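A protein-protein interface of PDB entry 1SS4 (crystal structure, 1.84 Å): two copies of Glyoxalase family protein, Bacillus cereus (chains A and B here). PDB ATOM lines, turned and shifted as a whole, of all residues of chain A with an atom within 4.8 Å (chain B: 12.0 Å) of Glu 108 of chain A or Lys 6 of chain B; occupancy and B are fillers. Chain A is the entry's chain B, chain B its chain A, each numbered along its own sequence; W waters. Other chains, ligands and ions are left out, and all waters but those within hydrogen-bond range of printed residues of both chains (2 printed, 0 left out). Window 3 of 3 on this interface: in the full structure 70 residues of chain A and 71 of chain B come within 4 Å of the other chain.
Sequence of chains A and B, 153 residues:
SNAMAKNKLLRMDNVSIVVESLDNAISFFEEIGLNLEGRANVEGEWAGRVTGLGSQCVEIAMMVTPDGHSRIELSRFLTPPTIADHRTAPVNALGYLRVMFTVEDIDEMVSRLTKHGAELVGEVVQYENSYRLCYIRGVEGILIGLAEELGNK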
ATOM      1  N   ASP A 105      -3.119  19.280  -1.939  1.00  0.00           N
ATOM      2  CA  ASP A 105      -2.945  18.176  -0.994  1.00  0.00           C
ATOM      3  C   ASP A 105      -3.626  16.920  -1.503  1.00  0.00           C
ATOM      4  O   ASP A 105      -4.829  16.784  -1.371  1.00  0.00           O
ATOM      5  CB  ASP A 105      -3.559  18.570   0.349  1.00  0.00           C
ATOM      6  CG  ASP A 105      -3.338  17.522   1.432  1.00  0.00           C
ATOM      7  OD1 ASP A 105      -3.015  16.356   1.124  1.00  0.00           O
ATOM      8  OD2 ASP A 105      -3.502  17.878   2.613  1.00  0.00           O
ATOM      9  N   ILE A 106      -2.858  15.997  -2.069  1.00  0.00           N
ATOM     10  CA  ILE A 106      -3.454  14.785  -2.625  1.00  0.00           C
ATOM     11  C   ILE A 106      -4.067  13.870  -1.575  1.00  0.00           C
ATOM     12  O   ILE A 106      -5.039  13.166  -1.841  1.00  0.00           O
ATOM     13  CB  ILE A 106      -2.420  14.024  -3.500  1.00  0.00           C
ATOM     14  CG1 ILE A 106      -3.137  12.998  -4.391  1.00  0.00           C
ATOM     15  CG2 ILE A 106      -1.344  13.363  -2.619  1.00  0.00           C
ATOM     16  CD1 ILE A 106      -2.263  12.437  -5.490  1.00  0.00           C
ATOM     17  N   ASP A 107      -3.525  13.884  -0.366  1.00  0.00           N
ATOM     18  CA  ASP A 107      -4.085  13.023   0.673  1.00  0.00           C
ATOM     19  C   ASP A 107      -5.499  13.441   1.058  1.00  0.00           C
ATOM     20  O   ASP A 107      -6.395  12.595   1.156  1.00  0.00           O
ATOM     21  CB  ASP A 107      -3.196  13.026   1.919  1.00  0.00           C
ATOM     22  CG  ASP A 107      -1.783  12.559   1.624  1.00  0.00           C
ATOM     23  OD1 ASP A 107      -1.604  11.416   1.147  1.00  0.00           O
ATOM     24  OD2 ASP A 107      -0.850  13.345   1.871  1.00  0.00           O
ATOM     25  N   GLU A 108      -5.700  14.740   1.262  1.00  0.00           N
ATOM     26  CA  GLU A 108      -7.010  15.259   1.648  1.00  0.00           C
ATOM     27  C   GLU A 108      -7.997  15.061   0.496  1.00  0.00           C
ATOM     28  O   GLU A 108      -9.156  14.734   0.715  1.00  0.00           O
ATOM     29  CB  GLU A 108      -6.894  16.741   2.009  1.00  0.00           C
ATOM     30  CG  GLU A 108      -8.144  17.394   2.626  1.00  0.00           C
ATOM     31  CD  GLU A 108      -9.218  17.813   1.617  1.00  0.00           C
ATOM     32  OE1 GLU A 108      -8.918  18.001   0.405  1.00  0.00           O
ATOM     33  OE2 GLU A 108     -10.381  17.974   2.053  1.00  0.00           O
ATOM     34  N   MET A 109      -7.542  15.260  -0.739  1.00  0.00           N
ATOM     35  CA  MET A 109      -8.451  15.070  -1.875  1.00  0.00           C
ATOM     36  C   MET A 109      -8.860  13.591  -2.015  1.00  0.00           C
ATOM     37  O   MET A 109     -10.029  13.294  -2.264  1.00  0.00           O
ATOM     38  CB  MET A 109      -7.807  15.562  -3.179  1.00  0.00           C
ATOM     39  CG  MET A 109      -8.741  15.459  -4.385  1.00  0.00           C
ATOM     40  SD  MET A 109     -10.396  16.500  -4.186  1.00  0.00           S
ATOM     41  CE  MET A 109      -9.682  18.284  -4.583  1.00  0.00           C
ATOM     42  N   VAL A 110      -7.914  12.662  -1.854  1.00  0.00           N
ATOM     43  CA  VAL A 110      -8.245  11.235  -1.977  1.00  0.00           C
ATOM     44  C   VAL A 110      -9.199  10.813  -0.879  1.00  0.00           C
ATOM     45  O   VAL A 110     -10.179  10.091  -1.130  1.00  0.00           O
ATOM     46  CB  VAL A 110      -6.983  10.334  -1.938  1.00  0.00           C
ATOM     47  CG1 VAL A 110      -7.377   8.871  -1.727  1.00  0.00           C
ATOM     48  CG2 VAL A 110      -6.205  10.486  -3.262  1.00  0.00           C
ATOM     49  N   SER A 111      -8.919  11.277   0.335  1.00  0.00           N
ATOM     50  CA  SER A 111      -9.768  10.944   1.462  1.00  0.00           C
ATOM     51  C   SER A 111     -11.199  11.474   1.265  1.00  0.00           C
ATOM     52  O   SER A 111     -12.171  10.745   1.465  1.00  0.00           O
ATOM     53  CB  SER A 111      -9.162  11.510   2.750  1.00  0.00           C
ATOM     54  OG  SER A 111      -9.970  11.163   3.866  1.00  0.00           O
ATOM     55  N   ARG A 112     -11.334  12.734   0.860  1.00  0.00           N
ATOM     56  CA  ARG A 112     -12.655  13.331   0.665  1.00  0.00           C
ATOM     57  C   ARG A 112     -13.441  12.658  -0.466  1.00  0.00           C
ATOM     58  O   ARG A 112     -14.631  12.321  -0.318  1.00  0.00           O
ATOM     59  CB  ARG A 112     -12.504  14.838   0.384  1.00  0.00           C
ATOM     60  CG  ARG A 112     -13.809  15.600   0.307  1.00  0.00           C
ATOM     61  CD  ARG A 112     -13.652  16.998   0.901  1.00  0.00           C
ATOM     62  NE  ARG A 112     -12.450  17.658   0.415  1.00  0.00           N
ATOM     63  CZ  ARG A 112     -12.332  18.194  -0.796  1.00  0.00           C
ATOM     64  NH1 ARG A 112     -13.358  18.146  -1.640  1.00  0.00           N
ATOM     65  NH2 ARG A 112     -11.194  18.776  -1.160  1.00  0.00           N
ATOM     66  N   ALA B   3     -14.419  27.449  -3.239  1.00  0.00           N
ATOM     67  CA  ALA B   3     -13.343  27.516  -2.215  1.00  0.00           C
ATOM     68  C   ALA B   3     -13.369  26.268  -1.332  1.00  0.00           C
ATOM     69  O   ALA B   3     -14.396  25.923  -0.740  1.00  0.00           O
ATOM     70  CB  ALA B   3     -13.514  28.775  -1.357  1.00  0.00           C
ATOM     71  N   MET B   4     -12.226  25.596  -1.253  1.00  0.00           N
ATOM     72  CA  MET B   4     -12.108  24.389  -0.450  1.00  0.00           C
ATOM     73  C   MET B   4     -11.276  24.659   0.793  1.00  0.00           C
ATOM     74  O   MET B   4     -10.124  25.085   0.705  1.00  0.00           O
ATOM     75  CB  MET B   4     -11.470  23.285  -1.279  1.00  0.00           C
ATOM     76  CG  MET B   4     -12.135  23.120  -2.622  1.00  0.00           C
ATOM     77  SD  MET B   4     -11.554  21.506  -3.469  1.00  0.00           S
ATOM     78  CE  MET B   4     -10.026  22.221  -4.461  1.00  0.00           C
ATOM     79  N   ALA B   5     -11.872  24.401   1.950  1.00  0.00           N
ATOM     80  CA  ALA B   5     -11.200  24.634   3.218  1.00  0.00           C
ATOM     81  C   ALA B   5      -9.792  24.046   3.289  1.00  0.00           C
ATOM     82  O   ALA B   5      -8.834  24.761   3.581  1.00  0.00           O
ATOM     83  CB  ALA B   5     -12.054  24.084   4.357  1.00  0.00           C
ATOM     84  N   LYS B   6      -9.664  22.752   3.011  1.00  0.00           N
ATOM     85  CA  LYS B   6      -8.367  22.088   3.101  1.00  0.00           C
ATOM     86  C   LYS B   6      -7.709  21.669   1.784  1.00  0.00           C
ATOM     87  O   LYS B   6      -7.067  20.610   1.712  1.00  0.00           O
ATOM     88  CB  LYS B   6      -8.480  20.856   4.000  1.00  0.00           C
ATOM     89  CG  LYS B   6      -8.951  21.127   5.414  1.00  0.00           C
ATOM     90  CD  LYS B   6      -8.896  19.831   6.227  1.00  0.00           C
ATOM     91  CE  LYS B   6      -9.234  20.055   7.698  1.00  0.00           C
ATOM     92  NZ  LYS B   6      -9.166  18.790   8.501  1.00  0.00           N
ATOM     93  N   ASN B   7      -7.855  22.483   0.748  1.00  0.00           N
ATOM     94  CA  ASN B   7      -7.231  22.145  -0.523  1.00  0.00           C
ATOM     95  C   ASN B   7      -7.338  23.245  -1.566  1.00  0.00           C
ATOM     96  O   ASN B   7      -7.970  24.271  -1.347  1.00  0.00           O
ATOM     97  CB  ASN B   7      -7.826  20.854  -1.086  1.00  0.00           C
ATOM     98  CG  ASN B   7      -6.759  19.897  -1.585  1.00  0.00           C
ATOM     99  OD1 ASN B   7      -5.781  20.310  -2.213  1.00  0.00           O
ATOM    100  ND2 ASN B   7      -6.941  18.608  -1.304  1.00  0.00           N
ATOM    101  N   LYS B   8      -6.716  23.014  -2.713  1.00  0.00           N
ATOM    102  CA  LYS B   8      -6.722  23.990  -3.790  1.00  0.00           C
ATOM    103  C   LYS B   8      -6.505  23.269  -5.114  1.00  0.00           C
ATOM    104  O   LYS B   8      -5.659  22.382  -5.207  1.00  0.00           O
ATOM    105  CB  LYS B   8      -5.605  25.012  -3.551  1.00  0.00           C
ATOM    106  CG  LYS B   8      -5.595  26.195  -4.495  1.00  0.00           C
ATOM    107  CD  LYS B   8      -4.537  27.206  -4.073  1.00  0.00           C
ATOM    108  CE  LYS B   8      -4.452  28.379  -5.050  1.00  0.00           C
ATOM    109  NZ  LYS B   8      -3.528  29.445  -4.544  1.00  0.00           N
ATOM    110  N   LEU B   9      -7.271  23.642  -6.135  1.00  0.00           N
ATOM    111  CA  LEU B   9      -7.122  23.022  -7.444  1.00  0.00           C
ATOM    112  C   LEU B   9      -6.222  23.950  -8.230  1.00  0.00           C
ATOM    113  O   LEU B   9      -6.664  25.029  -8.653  1.00  0.00           O
ATOM    114  CB  LEU B   9      -8.484  22.881  -8.138  1.00  0.00           C
ATOM    115  CG  LEU B   9      -8.475  22.201  -9.510  1.00  0.00           C
ATOM    116  CD1 LEU B   9      -7.855  20.813  -9.410  1.00  0.00           C
ATOM    117  CD2 LEU B   9      -9.896  22.118 -10.045  1.00  0.00           C
ATOM    118  N   LEU B  10      -4.973  23.533  -8.437  1.00  0.00           N
ATOM    119  CA  LEU B  10      -4.000  24.374  -9.141  1.00  0.00           C
ATOM    120  C   LEU B  10      -4.230  24.426 -10.648  1.00  0.00           C
ATOM    121  O   LEU B  10      -4.036  25.467 -11.272  1.00  0.00           O
ATOM    122  CB  LEU B  10      -2.577  23.920  -8.809  1.00  0.00           C
ATOM    123  CG  LEU B  10      -2.343  23.751  -7.290  1.00  0.00           C
ATOM    124  CD1 LEU B  10      -0.873  23.524  -7.045  1.00  0.00           C
ATOM    125  CD2 LEU B  10      -2.810  24.974  -6.528  1.00  0.00           C
HETATM  126  O   HOH W   1     -11.133  20.799   1.862  1.00  0.00           O
HETATM  127  O   HOH W   2      -4.965  20.001   3.346  1.00  0.00           O
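Asp 105 of chain A touches one residue of chain B. No residue of chain B comes within 4 Å of Ile 106 of chain A. Asp 107 of chain A touches none of the printed residues of chain B. Of chain B, only Lys 6 (3.5 Å) and Asn 7 (2.7 Å) come within 4 Å of Glu 108 of chain A. Of chain B, only Met 4 and Asn 7 come within 4 Å of Met 109 of chain A. No residue of chain B comes within 4 Å of Val 110 of chain A. No residue of chain B comes within 4 Å of Ser 111 of chain A. Arg 112 of chain A touches just these residues of chain B: Met 4 and Asn 7. Ala 3 of chain B touches none of the printed residues of chain A. Of the printed residues of chain A, Met 4 of chain B touches Met 109 (3.9 Å) and Arg 112 (3.6 Å). Lys 6 of chain B touches just one residue of chain A: Glu 108 (3.5 Å). Of the printed residues of chain A, Asn 7 of chain B touches Asp 105 (2.8 Å), Glu 108 (2.7 Å), Met 109 (3.4 Å) and Arg 112 (3.96 Å). The nearest residue of chain B that does not touch Glu 108 of chain A is Met 4 of chain B (5.9 Å). The nearest printed residue of chain A that does not touch Met 4 of chain B is Glu 108 of chain A (5.9 Å).
No position is printed for both chains.
Water W2 bridges the side-chain carboxylate (OD2) of Asp 105 of chain A and the backbone carbonyl oxygen (O) of Lys 6 of chain B. Water W1 lies within hydrogen-bond range of N of Lys 6 of chain B (2.7 Å) and OE2 of Glu 108 of chain A (2.9 Å).
Among the printed residues, merely in contact across the chains: Met 109 of chain A with Met 4 of chain B and Arg 112 of chain A with Asn 7 of chain B.
The guanidinium group (NH2) of Arg 112 of chain A is in hydrogen-bond range of the side-chain sulfur (SD) of Met 4 of chain B, 3.6 Å away. The backbone carbonyl oxygen (O) of Asp 105 of chain A is in hydrogen-bond range of the side-chain amide nitrogen (ND2) of Asn 7 of chain B (2.8 Å). The side-chain amide nitrogen (ND2) of Asn 7 of chain B lies within hydrogen-bond range of the side-chain carboxylate (OE1) of Glu 108 of chain A, at 2.7 Å. The side-chain amide nitrogen (ND2) of Asn 7 of chain B lies close to the backbone NH (N) of Met 109 of chain A, 3.4 Å away. The side-chain carboxylate of Glu 108 of chain A sits close to the backbone carbonyl oxygen of Lys 6 of chain B (3.5 Å).
The side-chain carboxylate of Asp 105 of chain A sits at hydrogen-bond distance from the backbone NH of Asp 107 of chain A, at 2.9 Å. OD1 of Asp 105 of chain A lies within hydrogen-bond range of N of Glu 108 of chain A (3.1 Å). NE of Arg 112 of chain A is in salt-bridge range of OE2 of Glu 108 of chain A (2.7 Å).
Of the 8 printed residues of chain A, 4 touch a printed residue of chain B. Printed residues of chain A that touch a printed residue of chain B: Asp 105, Glu 108, Met 109 and Arg 112. Hydrophobic or aromatic side chains of chain A that line the printed part of chain B: Met 109. Along chain A the printed residues that touch a printed residue of chain B span positions 105 to 112. Of the 8 printed residues of chain B, 3 touch a printed residue of chain A. Printed residues of chain B that touch a printed residue of chain A: Met 4, Lys 6 and Asn 7.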
